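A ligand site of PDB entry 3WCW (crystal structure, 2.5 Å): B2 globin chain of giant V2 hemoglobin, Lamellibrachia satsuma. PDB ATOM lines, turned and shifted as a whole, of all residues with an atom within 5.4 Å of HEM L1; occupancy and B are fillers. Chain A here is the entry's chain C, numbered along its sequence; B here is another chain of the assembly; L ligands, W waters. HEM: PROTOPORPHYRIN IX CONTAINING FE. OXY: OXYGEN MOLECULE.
Water W1 lies within hydrogen-bond range of NE of Arg 70, ND1 of His 67 and O2D of HEM L1.
Residues that only touch HEM L1: Leu 50 (3.4 Å), Phe 51 (3.4 Å), Val 54 (3.6 Å), His 67 (3.8 Å), Arg 70 (3.1 Å), Val 71 (3.5 Å), Leu 75 (3.7 Å), Gln 98 (3.4 Å), Arg 102 (3.7 Å), Val 105 (3.9 Å), Gly 109 (3.7 Å), Phe 110 (3.4 Å), Ile 113 (3.8 Å), Thr 141 (3.8 Å) and Met 144 (3.5 Å). Hydrophobic or aromatic side chains within 4 Å of HEM L1: Leu 50, Phe 51, Val 54, His 67, Val 71, Leu 75, His 99, Val 105, Phe 110, Ile 113, Met 144 and His 90 of chain B. Of the 27 residues printed, 19 come within 4 Å of HEM L1.
An iron atom (FE) of HEM L1 is bound by an oxygen (O1) of OXY L2 (1.8 Å).
A ring nitrogen (NE2) of His 67 sits at hydrogen-bond distance from an oxygen (O2) of OXY L2, at 2.9 Å. The guanidinium group (NE) of Arg 53 is in salt-bridge range of an oxygen (O1D) of HEM L1 (2.7 Å). NE2 of His 99 is bound to FE of HEM L1, at 2.1 Å. A ring nitrogen (NE2) of His 90 of chain B is in hydrogen-bond range of an oxygen (O1A) of HEM L1 (2.9 Å). The side-chain amide nitrogen (NE2) of Gln 94 of chain B lies within hydrogen-bond range of an oxygen (O1A) of HEM L1, at 3.2 Å. O1A of HEM L3 lies within hydrogen-bond range of NE2 of Gln 98, 3.2 Å away.
The side-chain amide nitrogen of Gln 94 of chain B lies within hydrogen-bond range of a ring nitrogen (NE2) of His 90 of chain B (3.5 Å). O of Gln 98 lies within hydrogen-bond range of NE of Arg 102 (2.7 Å). O of Leu 95 is in hydrogen-bond range of ND1 of His 99, 2.8 Å away. OG1 of Thr 141 is in hydrogen-bond range of O of Phe 137, 3.5 Å away.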
ATOM      1  N   LEU A  40       4.850 -35.468  16.249  1.00  0.00           N
ATOM      2  CA  LEU A  40       5.813 -35.859  17.275  1.00  0.00           C
ATOM      3  C   LEU A  40       5.207 -36.924  18.187  1.00  0.00           C
ATOM      4  O   LEU A  40       5.823 -37.958  18.478  1.00  0.00           O
ATOM      5  CB  LEU A  40       6.222 -34.630  18.118  1.00  0.00           C
ATOM      6  CG  LEU A  40       7.193 -34.905  19.274  1.00  0.00           C
ATOM      7  CD1 LEU A  40       8.483 -35.475  18.730  1.00  0.00           C
ATOM      8  CD2 LEU A  40       7.462 -33.625  20.056  1.00  0.00           C
ATOM      9  N   LEU A  50       4.590 -34.865  28.541  1.00  0.00           N
ATOM     10  CA  LEU A  50       5.426 -33.737  28.957  1.00  0.00           C
ATOM     11  C   LEU A  50       4.639 -32.434  28.850  1.00  0.00           C
ATOM     12  O   LEU A  50       5.076 -31.397  29.338  1.00  0.00           O
ATOM     13  CB  LEU A  50       6.671 -33.637  28.082  1.00  0.00           C
ATOM     14  CG  LEU A  50       7.560 -34.886  27.985  1.00  0.00           C
ATOM     15  CD1 LEU A  50       8.523 -34.724  26.820  1.00  0.00           C
ATOM     16  CD2 LEU A  50       8.307 -35.084  29.288  1.00  0.00           C
ATOM     17  N   PHE A  51       3.458 -32.510  28.223  1.00  0.00           N
ATOM     18  CA  PHE A  51       2.632 -31.328  28.013  1.00  0.00           C
ATOM     19  C   PHE A  51       1.283 -31.421  28.720  1.00  0.00           C
ATOM     20  O   PHE A  51       0.249 -30.921  28.241  1.00  0.00           O
ATOM     21  CB  PHE A  51       2.443 -31.131  26.503  1.00  0.00           C
ATOM     22  CG  PHE A  51       3.746 -31.171  25.736  1.00  0.00           C
ATOM     23  CD1 PHE A  51       4.572 -30.050  25.680  1.00  0.00           C
ATOM     24  CD2 PHE A  51       4.180 -32.361  25.139  1.00  0.00           C
ATOM     25  CE1 PHE A  51       5.813 -30.117  25.054  1.00  0.00           C
ATOM     26  CE2 PHE A  51       5.418 -32.437  24.515  1.00  0.00           C
ATOM     27  CZ  PHE A  51       6.245 -31.304  24.467  1.00  0.00           C
ATOM     28  N   ARG A  53       0.471 -29.958  31.461  1.00  0.00           N
ATOM     29  CA  ARG A  53       0.116 -28.617  31.910  1.00  0.00           C
ATOM     30  C   ARG A  53      -0.590 -27.775  30.822  1.00  0.00           C
ATOM     31  O   ARG A  53      -1.351 -26.864  31.142  1.00  0.00           O
ATOM     32  CB  ARG A  53       1.375 -27.891  32.402  1.00  0.00           C
ATOM     33  CG  ARG A  53       1.102 -26.774  33.383  1.00  0.00           C
ATOM     34  CD  ARG A  53       2.273 -25.850  33.441  1.00  0.00           C
ATOM     35  NE  ARG A  53       2.398 -25.107  32.191  1.00  0.00           N
ATOM     36  CZ  ARG A  53       1.639 -24.074  31.853  1.00  0.00           C
ATOM     37  NH1 ARG A  53       1.819 -23.474  30.681  1.00  0.00           N
ATOM     38  NH2 ARG A  53       0.713 -23.614  32.683  1.00  0.00           N
ATOM     39  N   VAL A  54      -0.329 -28.074  29.552  1.00  0.00           N
ATOM     40  CA  VAL A  54      -0.941 -27.354  28.439  1.00  0.00           C
ATOM     41  C   VAL A  54      -1.972 -28.219  27.701  1.00  0.00           C
ATOM     42  O   VAL A  54      -2.374 -27.909  26.583  1.00  0.00           O
ATOM     43  CB  VAL A  54       0.133 -26.884  27.418  1.00  0.00           C
ATOM     44  CG1 VAL A  54       1.026 -25.822  28.050  1.00  0.00           C
ATOM     45  CG2 VAL A  54       0.968 -28.061  26.948  1.00  0.00           C
ATOM     46  N   HIS A  67      -0.215 -22.812  23.860  1.00  0.00           N
ATOM     47  CA  HIS A  67       1.131 -23.363  23.919  1.00  0.00           C
ATOM     48  C   HIS A  67       1.780 -23.410  22.525  1.00  0.00           C
ATOM     49  O   HIS A  67       2.936 -23.012  22.356  1.00  0.00           O
ATOM     50  CB  HIS A  67       1.084 -24.764  24.519  1.00  0.00           C
ATOM     51  CG  HIS A  67       2.379 -25.499  24.394  1.00  0.00           C
ATOM     52  ND1 HIS A  67       3.513 -25.129  25.076  1.00  0.00           N
ATOM     53  CD2 HIS A  67       2.719 -26.565  23.634  1.00  0.00           C
ATOM     54  CE1 HIS A  67       4.510 -25.936  24.733  1.00  0.00           C
ATOM     55  NE2 HIS A  67       4.053 -26.817  23.868  1.00  0.00           N
ATOM     56  N   ARG A  70       2.918 -20.167  21.449  1.00  0.00           N
ATOM     57  CA  ARG A  70       4.183 -19.811  22.117  1.00  0.00           C
ATOM     58  C   ARG A  70       5.355 -20.556  21.478  1.00  0.00           C
ATOM     59  O   ARG A  70       6.445 -19.993  21.339  1.00  0.00           O
ATOM     60  CB  ARG A  70       4.137 -20.126  23.632  1.00  0.00           C
ATOM     61  CG  ARG A  70       3.186 -19.231  24.433  1.00  0.00           C
ATOM     62  CD  ARG A  70       3.351 -19.406  25.944  1.00  0.00           C
ATOM     63  NE  ARG A  70       2.889 -20.708  26.460  1.00  0.00           N
ATOM     64  CZ  ARG A  70       1.619 -21.021  26.713  1.00  0.00           C
ATOM     65  NH1 ARG A  70       0.657 -20.131  26.507  1.00  0.00           N
ATOM     66  NH2 ARG A  70       1.319 -22.238  27.166  1.00  0.00           N
ATOM     67  N   VAL A  71       5.158 -21.811  21.101  1.00  0.00           N
ATOM     68  CA  VAL A  71       6.241 -22.548  20.475  1.00  0.00           C
ATOM     69  C   VAL A  71       6.621 -21.882  19.157  1.00  0.00           C
ATOM     70  O   VAL A  71       7.791 -21.605  18.894  1.00  0.00           O
ATOM     71  CB  VAL A  71       5.854 -24.011  20.208  1.00  0.00           C
ATOM     72  CG1 VAL A  71       6.997 -24.719  19.450  1.00  0.00           C
ATOM     73  CG2 VAL A  71       5.582 -24.713  21.524  1.00  0.00           C
ATOM     74  N   GLY A  74       8.319 -18.563  19.553  1.00  0.00           N
ATOM     75  CA  GLY A  74       9.708 -18.772  19.923  1.00  0.00           C
ATOM     76  C   GLY A  74      10.578 -19.178  18.745  1.00  0.00           C
ATOM     77  O   GLY A  74      11.745 -18.769  18.668  1.00  0.00           O
ATOM     78  N   LEU A  75      10.027 -19.978  17.852  1.00  0.00           N
ATOM     79  CA  LEU A  75      10.772 -20.417  16.678  1.00  0.00           C
ATOM     80  C   LEU A  75      10.869 -19.233  15.691  1.00  0.00           C
ATOM     81  O   LEU A  75      11.876 -19.067  14.995  1.00  0.00           O
ATOM     82  CB  LEU A  75      10.062 -21.608  16.009  1.00  0.00           C
ATOM     83  CG  LEU A  75      10.846 -22.092  14.791  1.00  0.00           C
ATOM     84  CD1 LEU A  75      12.243 -22.494  15.222  1.00  0.00           C
ATOM     85  CD2 LEU A  75      10.129 -23.249  14.112  1.00  0.00           C
ATOM     86  N   LEU A  95      15.822 -19.845  26.204  1.00  0.00           N
ATOM     87  CA  LEU A  95      14.937 -20.937  25.812  1.00  0.00           C
ATOM     88  C   LEU A  95      15.438 -22.218  26.445  1.00  0.00           C
ATOM     89  O   LEU A  95      14.671 -23.106  26.801  1.00  0.00           O
ATOM     90  CB  LEU A  95      14.875 -21.084  24.286  1.00  0.00           C
ATOM     91  CG  LEU A  95      14.044 -20.020  23.548  1.00  0.00           C
ATOM     92  CD1 LEU A  95      14.284 -20.138  22.052  1.00  0.00           C
ATOM     93  CD2 LEU A  95      12.578 -20.214  23.870  1.00  0.00           C
ATOM     94  N   GLN A  98      14.418 -22.629  29.904  1.00  0.00           N
ATOM     95  CA  GLN A  98      12.975 -22.872  29.928  1.00  0.00           C
ATOM     96  C   GLN A  98      12.689 -24.362  29.697  1.00  0.00           C
ATOM     97  O   GLN A  98      11.672 -24.870  30.162  1.00  0.00           O
ATOM     98  CB  GLN A  98      12.251 -22.061  28.865  1.00  0.00           C
ATOM     99  CG  GLN A  98      12.158 -20.564  29.147  1.00  0.00           C
ATOM    100  CD  GLN A  98      11.218 -19.849  28.203  1.00  0.00           C
ATOM    101  OE1 GLN A  98      11.256 -20.075  26.998  1.00  0.00           O
ATOM    102  NE2 GLN A  98      10.388 -18.983  28.741  1.00  0.00           N
ATOM    103  N   HIS A  99      13.589 -25.033  28.988  1.00  0.00           N
ATOM    104  CA  HIS A  99      13.400 -26.452  28.705  1.00  0.00           C
ATOM    105  C   HIS A  99      14.154 -27.347  29.669  1.00  0.00           C
ATOM    106  O   HIS A  99      14.024 -28.575  29.634  1.00  0.00           O
ATOM    107  CB  HIS A  99      13.810 -26.757  27.256  1.00  0.00           C
ATOM    108  CG  HIS A  99      12.850 -26.234  26.240  1.00  0.00           C
ATOM    109  ND1 HIS A  99      12.743 -24.892  25.940  1.00  0.00           N
ATOM    110  CD2 HIS A  99      11.899 -26.857  25.510  1.00  0.00           C
ATOM    111  CE1 HIS A  99      11.763 -24.709  25.078  1.00  0.00           C
ATOM    112  NE2 HIS A  99      11.232 -25.892  24.797  1.00  0.00           N
ATOM    113  N   ARG A 102      12.960 -29.912  33.512  1.00  0.00           N
ATOM    114  CA  ARG A 102      11.735 -30.548  33.057  1.00  0.00           C
ATOM    115  C   ARG A 102      12.215 -31.902  32.583  1.00  0.00           C
ATOM    116  O   ARG A 102      12.671 -32.054  31.451  1.00  0.00           O
ATOM    117  CB  ARG A 102      11.115 -29.777  31.888  1.00  0.00           C
ATOM    118  CG  ARG A 102      10.572 -28.415  32.243  1.00  0.00           C
ATOM    119  CD  ARG A 102       9.973 -27.752  31.010  1.00  0.00           C
ATOM    120  NE  ARG A 102       9.659 -26.338  31.218  1.00  0.00           N
ATOM    121  CZ  ARG A 102       8.657 -25.881  31.960  1.00  0.00           C
ATOM    122  NH1 ARG A 102       8.466 -24.568  32.070  1.00  0.00           N
ATOM    123  NH2 ARG A 102       7.849 -26.728  32.591  1.00  0.00           N
ATOM    124  N   GLY A 104      12.628 -35.571  31.129  1.00  0.00           N
ATOM    125  CA  GLY A 104      12.069 -36.092  29.904  1.00  0.00           C
ATOM    126  C   GLY A 104      12.501 -35.300  28.690  1.00  0.00           C
ATOM    127  O   GLY A 104      12.924 -35.867  27.696  1.00  0.00           O
ATOM    128  N   VAL A 105      12.398 -33.973  28.782  1.00  0.00           N
ATOM    129  CA  VAL A 105      12.809 -33.084  27.698  1.00  0.00           C
ATOM    130  C   VAL A 105      14.303 -33.261  27.473  1.00  0.00           C
ATOM    131  O   VAL A 105      15.106 -32.752  28.256  1.00  0.00           O
ATOM    132  CB  VAL A 105      12.552 -31.615  28.050  1.00  0.00           C
ATOM    133  CG1 VAL A 105      13.024 -30.715  26.922  1.00  0.00           C
ATOM    134  CG2 VAL A 105      11.073 -31.399  28.352  1.00  0.00           C
ATOM    135  N   THR A 106      14.675 -33.962  26.397  1.00  0.00           N
ATOM    136  CA  THR A 106      16.083 -34.213  26.101  1.00  0.00           C
ATOM    137  C   THR A 106      16.460 -33.942  24.650  1.00  0.00           C
ATOM    138  O   THR A 106      15.619 -33.570  23.830  1.00  0.00           O
ATOM    139  CB  THR A 106      16.431 -35.681  26.395  1.00  0.00           C
ATOM    140  OG1 THR A 106      15.782 -36.528  25.433  1.00  0.00           O
ATOM    141  CG2 THR A 106      15.953 -36.062  27.781  1.00  0.00           C
ATOM    142  N   GLY A 109      14.235 -35.698  22.122  1.00  0.00           N
ATOM    143  CA  GLY A 109      12.982 -35.128  21.688  1.00  0.00           C
ATOM    144  C   GLY A 109      13.152 -34.106  20.576  1.00  0.00           C
ATOM    145  O   GLY A 109      12.346 -34.044  19.641  1.00  0.00           O
ATOM    146  N   PHE A 110      14.205 -33.290  20.671  1.00  0.00           N
ATOM    147  CA  PHE A 110      14.461 -32.276  19.672  1.00  0.00           C
ATOM    148  C   PHE A 110      14.820 -32.915  18.338  1.00  0.00           C
ATOM    149  O   PHE A 110      14.445 -32.396  17.289  1.00  0.00           O
ATOM    150  CB  PHE A 110      15.577 -31.338  20.137  1.00  0.00           C
ATOM    151  CG  PHE A 110      15.113 -30.301  21.132  1.00  0.00           C
ATOM    152  CD1 PHE A 110      14.809 -29.015  20.713  1.00  0.00           C
ATOM    153  CD2 PHE A 110      14.944 -30.636  22.471  1.00  0.00           C
ATOM    154  CE1 PHE A 110      14.336 -28.066  21.624  1.00  0.00           C
ATOM    155  CE2 PHE A 110      14.474 -29.697  23.396  1.00  0.00           C
ATOM    156  CZ  PHE A 110      14.169 -28.410  22.977  1.00  0.00           C
ATOM    157  N   ILE A 113      11.457 -33.849  17.012  1.00  0.00           N
ATOM    158  CA  ILE A 113      10.662 -32.751  16.504  1.00  0.00           C
ATOM    159  C   ILE A 113      11.264 -32.225  15.190  1.00  0.00           C
ATOM    160  O   ILE A 113      10.534 -31.757  14.305  1.00  0.00           O
ATOM    161  CB  ILE A 113      10.507 -31.618  17.556  1.00  0.00           C
ATOM    162  CG1 ILE A 113       9.212 -30.860  17.287  1.00  0.00           C
ATOM    163  CG2 ILE A 113      11.718 -30.680  17.535  1.00  0.00           C
ATOM    164  CD1 ILE A 113       8.799 -29.946  18.407  1.00  0.00           C
ATOM    165  N   PHE A 117       9.126 -31.492  11.874  1.00  0.00           N
ATOM    166  CA  PHE A 117       9.117 -30.276  11.068  1.00  0.00           C
ATOM    167  C   PHE A 117       9.482 -30.605   9.626  1.00  0.00           C
ATOM    168  O   PHE A 117       8.924 -30.044   8.689  1.00  0.00           O
ATOM    169  CB  PHE A 117      10.081 -29.243  11.647  1.00  0.00           C
ATOM    170  CG  PHE A 117       9.418 -28.245  12.551  1.00  0.00           C
ATOM    171  CD1 PHE A 117       8.676 -27.196  12.023  1.00  0.00           C
ATOM    172  CD2 PHE A 117       9.504 -28.375  13.930  1.00  0.00           C
ATOM    173  CE1 PHE A 117       8.033 -26.284  12.858  1.00  0.00           C
ATOM    174  CE2 PHE A 117       8.877 -27.468  14.780  1.00  0.00           C
ATOM    175  CZ  PHE A 117       8.137 -26.421  14.243  1.00  0.00           C
ATOM    176  N   PHE A 137      17.950 -25.304  11.480  1.00  0.00           N
ATOM    177  CA  PHE A 137      17.041 -25.750  12.537  1.00  0.00           C
ATOM    178  C   PHE A 137      17.937 -26.321  13.636  1.00  0.00           C
ATOM    179  O   PHE A 137      17.794 -25.968  14.800  1.00  0.00           O
ATOM    180  CB  PHE A 137      16.094 -26.856  12.032  1.00  0.00           C
ATOM    181  CG  PHE A 137      14.967 -27.171  12.983  1.00  0.00           C
ATOM    182  CD1 PHE A 137      13.787 -26.422  12.959  1.00  0.00           C
ATOM    183  CD2 PHE A 137      15.093 -28.183  13.929  1.00  0.00           C
ATOM    184  CE1 PHE A 137      12.754 -26.674  13.861  1.00  0.00           C
ATOM    185  CE2 PHE A 137      14.056 -28.445  14.832  1.00  0.00           C
ATOM    186  CZ  PHE A 137      12.889 -27.690  14.809  1.00  0.00           C
ATOM    187  N   ILE A 140      19.790 -23.888  15.549  1.00  0.00           N
ATOM    188  CA  ILE A 140      18.853 -23.344  16.523  1.00  0.00           C
ATOM    189  C   ILE A 140      18.656 -24.285  17.724  1.00  0.00           C
ATOM    190  O   ILE A 140      18.762 -23.844  18.872  1.00  0.00           O
ATOM    191  CB  ILE A 140      17.466 -23.048  15.880  1.00  0.00           C
ATOM    192  CG1 ILE A 140      17.586 -21.870  14.919  1.00  0.00           C
ATOM    193  CG2 ILE A 140      16.426 -22.771  16.974  1.00  0.00           C
ATOM    194  CD1 ILE A 140      16.282 -21.451  14.303  1.00  0.00           C
ATOM    195  N   THR A 141      18.386 -25.555  17.463  1.00  0.00           N
ATOM    196  CA  THR A 141      18.173 -26.494  18.566  1.00  0.00           C
ATOM    197  C   THR A 141      19.396 -26.656  19.459  1.00  0.00           C
ATOM    198  O   THR A 141      19.275 -26.722  20.679  1.00  0.00           O
ATOM    199  CB  THR A 141      17.690 -27.894  18.097  1.00  0.00           C
ATOM    200  OG1 THR A 141      18.601 -28.435  17.138  1.00  0.00           O
ATOM    201  CG2 THR A 141      16.276 -27.811  17.491  1.00  0.00           C
ATOM    202  N   MET A 144      19.436 -24.596  22.237  1.00  0.00           N
ATOM    203  CA  MET A 144      18.334 -24.872  23.152  1.00  0.00           C
ATOM    204  C   MET A 144      18.564 -26.136  23.981  1.00  0.00           C
ATOM    205  O   MET A 144      18.024 -26.263  25.071  1.00  0.00           O
ATOM    206  CB  MET A 144      17.023 -25.014  22.391  1.00  0.00           C
ATOM    207  CG  MET A 144      16.577 -23.766  21.640  1.00  0.00           C
ATOM    208  SD  MET A 144      15.093 -24.124  20.647  1.00  0.00           S
ATOM    209  CE  MET A 144      13.848 -24.083  21.907  1.00  0.00           C
ATOM    210  N   HIS B  90      -1.042 -16.409  30.730  1.00  0.00           N
ATOM    211  CA  HIS B  90       0.341 -16.886  30.799  1.00  0.00           C
ATOM    212  C   HIS B  90       1.230 -15.679  31.101  1.00  0.00           C
ATOM    213  O   HIS B  90       1.978 -15.666  32.069  1.00  0.00           O
ATOM    214  CB  HIS B  90       0.748 -17.512  29.471  1.00  0.00           C
ATOM    215  CG  HIS B  90       2.019 -18.304  29.544  1.00  0.00           C
ATOM    216  ND1 HIS B  90       2.049 -19.637  29.890  1.00  0.00           N
ATOM    217  CD2 HIS B  90       3.304 -17.969  29.268  1.00  0.00           C
ATOM    218  CE1 HIS B  90       3.285 -20.084  29.819  1.00  0.00           C
ATOM    219  NE2 HIS B  90       4.074 -19.087  29.451  1.00  0.00           N
ATOM    220  N   GLN B  94       4.021 -14.743  34.150  1.00  0.00           N
ATOM    221  CA  GLN B  94       5.401 -14.337  33.948  1.00  0.00           C
ATOM    222  C   GLN B  94       5.728 -13.012  34.626  1.00  0.00           C
ATOM    223  O   GLN B  94       6.894 -12.691  34.822  1.00  0.00           O
ATOM    224  CB  GLN B  94       5.707 -14.321  32.441  1.00  0.00           C
ATOM    225  CG  GLN B  94       5.423 -15.675  31.768  1.00  0.00           C
ATOM    226  CD  GLN B  94       5.589 -15.690  30.242  1.00  0.00           C
ATOM    227  OE1 GLN B  94       4.938 -14.919  29.528  1.00  0.00           O
ATOM    228  NE2 GLN B  94       6.461 -16.555  29.754  1.00  0.00           N
HETATM  229  CHA HEM L   1       7.754 -24.781  26.422  1.00  0.00           C
HETATM  230  CHB HEM L   1       9.573 -23.371  22.293  1.00  0.00           C
HETATM  231  CHC HEM L   1      10.913 -27.895  21.292  1.00  0.00           C
HETATM  232  CHD HEM L   1       9.107 -29.264  25.507  1.00  0.00           C
HETATM  233  C1A HEM L   1       8.127 -23.977  25.393  1.00  0.00           C
HETATM  234  C2A HEM L   1       7.869 -22.605  25.350  1.00  0.00           C
HETATM  235  C3A HEM L   1       8.393 -22.175  24.181  1.00  0.00           C
HETATM  236  C4A HEM L   1       8.982 -23.328  23.479  1.00  0.00           C
HETATM  237  CMA HEM L   1       8.390 -20.735  23.614  1.00  0.00           C
HETATM  238  CAA HEM L   1       7.146 -21.765  26.407  1.00  0.00           C
HETATM  239  CBA HEM L   1       8.049 -21.201  27.458  1.00  0.00           C
HETATM  240  CGA HEM L   1       7.319 -20.368  28.526  1.00  0.00           C
HETATM  241  O1A HEM L   1       6.654 -19.353  28.189  1.00  0.00           O
HETATM  242  O2A HEM L   1       7.402 -20.746  29.662  1.00  0.00           O
HETATM  243  C1B HEM L   1      10.120 -24.481  21.604  1.00  0.00           C
HETATM  244  C2B HEM L   1      10.735 -24.413  20.291  1.00  0.00           C
HETATM  245  C3B HEM L   1      11.123 -25.773  20.010  1.00  0.00           C
HETATM  246  C4B HEM L   1      10.727 -26.527  21.148  1.00  0.00           C
HETATM  247  CMB HEM L   1      10.902 -23.190  19.454  1.00  0.00           C
HETATM  248  CAB HEM L   1      11.771 -26.189  18.781  1.00  0.00           C
HETATM  249  CBB HEM L   1      13.055 -26.016  18.523  1.00  0.00           C
HETATM  250  C1C HEM L   1      10.541 -28.659  22.373  1.00  0.00           C
HETATM  251  C2C HEM L   1      10.785 -30.110  22.434  1.00  0.00           C
HETATM  252  C3C HEM L   1      10.257 -30.559  23.670  1.00  0.00           C
HETATM  253  C4C HEM L   1       9.714 -29.284  24.298  1.00  0.00           C
HETATM  254  CMC HEM L   1      11.468 -30.937  21.344  1.00  0.00           C
HETATM  255  CAC HEM L   1      10.236 -31.843  24.183  1.00  0.00           C
HETATM  256  CBC HEM L   1      10.583 -33.068  23.882  1.00  0.00           C
HETATM  257  C1D HEM L   1       8.567 -28.155  26.135  1.00  0.00           C
HETATM  258  C2D HEM L   1       7.876 -28.197  27.480  1.00  0.00           C
HETATM  259  C3D HEM L   1       7.504 -26.899  27.695  1.00  0.00           C
HETATM  260  C4D HEM L   1       7.949 -26.112  26.548  1.00  0.00           C
HETATM  261  CMD HEM L   1       7.681 -29.450  28.329  1.00  0.00           C
HETATM  262  CAD HEM L   1       6.741 -26.330  28.874  1.00  0.00           C
HETATM  263  CBD HEM L   1       5.284 -26.268  28.506  1.00  0.00           C
HETATM  264  CGD HEM L   1       4.436 -25.688  29.531  1.00  0.00           C
HETATM  265  O1D HEM L   1       4.102 -26.380  30.539  1.00  0.00           O
HETATM  266  O2D HEM L   1       4.062 -24.512  29.398  1.00  0.00           O
HETATM  267  NA  HEM L   1       8.809 -24.437  24.255  1.00  0.00           N
HETATM  268  NB  HEM L   1      10.097 -25.708  22.124  1.00  0.00           N
HETATM  269  NC  HEM L   1       9.901 -28.205  23.511  1.00  0.00           N
HETATM  270  ND  HEM L   1       8.583 -26.900  25.638  1.00  0.00           N
HETATM  271 FE   HEM L   1       9.366 -26.313  23.894  1.00  0.00          FE
HETATM  272  O1  OXY L   2       7.753 -26.653  23.144  1.00  0.00           O
HETATM  273  O2  OXY L   2       6.773 -27.406  23.226  1.00  0.00           O
HETATM  274  CHA HEM L   3       9.375 -10.320  31.107  1.00  0.00           C
HETATM  275  CHB HEM L   3       5.937  -9.513  27.973  1.00  0.00           C
HETATM  276  CHC HEM L   3       4.949  -5.283  30.058  1.00  0.00           C
HETATM  277  CHD HEM L   3       8.492  -6.121  33.209  1.00  0.00           C
HETATM  278  C1A HEM L   3       8.527 -10.478  30.061  1.00  0.00           C
HETATM  279  C2A HEM L   3       8.545 -11.604  29.222  1.00  0.00           C
HETATM  280  C3A HEM L   3       7.577 -11.389  28.323  1.00  0.00           C
HETATM  281  C4A HEM L   3       6.945 -10.110  28.608  1.00  0.00           C
HETATM  282  CMA HEM L   3       7.166 -12.318  27.154  1.00  0.00           C
HETATM  283  CAA HEM L   3       9.466 -12.805  29.308  1.00  0.00           C
HETATM  284  CBA HEM L   3       8.974 -13.841  30.288  1.00  0.00           C
HETATM  285  CGA HEM L   3       9.897 -15.049  30.397  1.00  0.00           C
HETATM  286  O1A HEM L   3      10.001 -15.828  29.416  1.00  0.00           O
HETATM  287  O2A HEM L   3      10.513 -15.191  31.421  1.00  0.00           O
HETATM  288  C1B HEM L   3       5.333  -8.280  28.254  1.00  0.00           C
HETATM  289  C2B HEM L   3       4.235  -7.734  27.479  1.00  0.00           C
HETATM  290  C3B HEM L   3       3.938  -6.476  28.116  1.00  0.00           C
HETATM  291  C4B HEM L   3       4.873  -6.364  29.180  1.00  0.00           C
HETATM  292  CMB HEM L   3       3.578  -8.359  26.302  1.00  0.00           C
HETATM  293  CAB HEM L   3       2.900  -5.595  27.657  1.00  0.00           C
HETATM  294  CBB HEM L   3       3.116  -4.471  27.022  1.00  0.00           C
HETATM  295  C1C HEM L   3       5.845  -5.147  31.098  1.00  0.00           C
HETATM  296  C2C HEM L   3       5.877  -3.960  31.963  1.00  0.00           C
HETATM  297  C3C HEM L   3       6.905  -4.163  32.902  1.00  0.00           C
HETATM  298  C4C HEM L   3       7.462  -5.521  32.538  1.00  0.00           C
HETATM  299  CMC HEM L   3       4.948  -2.740  31.849  1.00  0.00           C
HETATM  300  CAC HEM L   3       7.300  -3.322  33.891  1.00  0.00           C
HETATM  301  CBC HEM L   3       7.871  -2.164  33.997  1.00  0.00           C
HETATM  302  C1D HEM L   3       9.043  -7.355  32.919  1.00  0.00           C
HETATM  303  C2D HEM L   3      10.186  -7.987  33.693  1.00  0.00           C
HETATM  304  C3D HEM L   3      10.404  -9.175  33.075  1.00  0.00           C
HETATM  305  C4D HEM L   3       9.444  -9.273  31.961  1.00  0.00           C
HETATM  306  CMD HEM L   3      10.877  -7.373  34.889  1.00  0.00           C
HETATM  307  CAD HEM L   3      11.429 -10.220  33.436  1.00  0.00           C
HETATM  308  CBD HEM L   3      12.655 -10.173  32.591  1.00  0.00           C
HETATM  309  CGD HEM L   3      13.608 -11.218  32.970  1.00  0.00           C
HETATM  310  O1D HEM L   3      13.591 -12.346  32.366  1.00  0.00           O
HETATM  311  O2D HEM L   3      14.421 -10.989  33.886  1.00  0.00           O
HETATM  312  NA  HEM L   3       7.557  -9.544  29.707  1.00  0.00           N
HETATM  313  NB  HEM L   3       5.724  -7.490  29.265  1.00  0.00           N
HETATM  314  NC  HEM L   3       6.817  -6.056  31.478  1.00  0.00           N
HETATM  315  ND  HEM L   3       8.643  -8.164  31.910  1.00  0.00           N
HETATM  316 FE   HEM L   3       7.184  -7.803  30.598  1.00  0.00          FE
HETATM  317  O   HOH W   1       3.948 -23.179  26.951  1.00  0.00           O
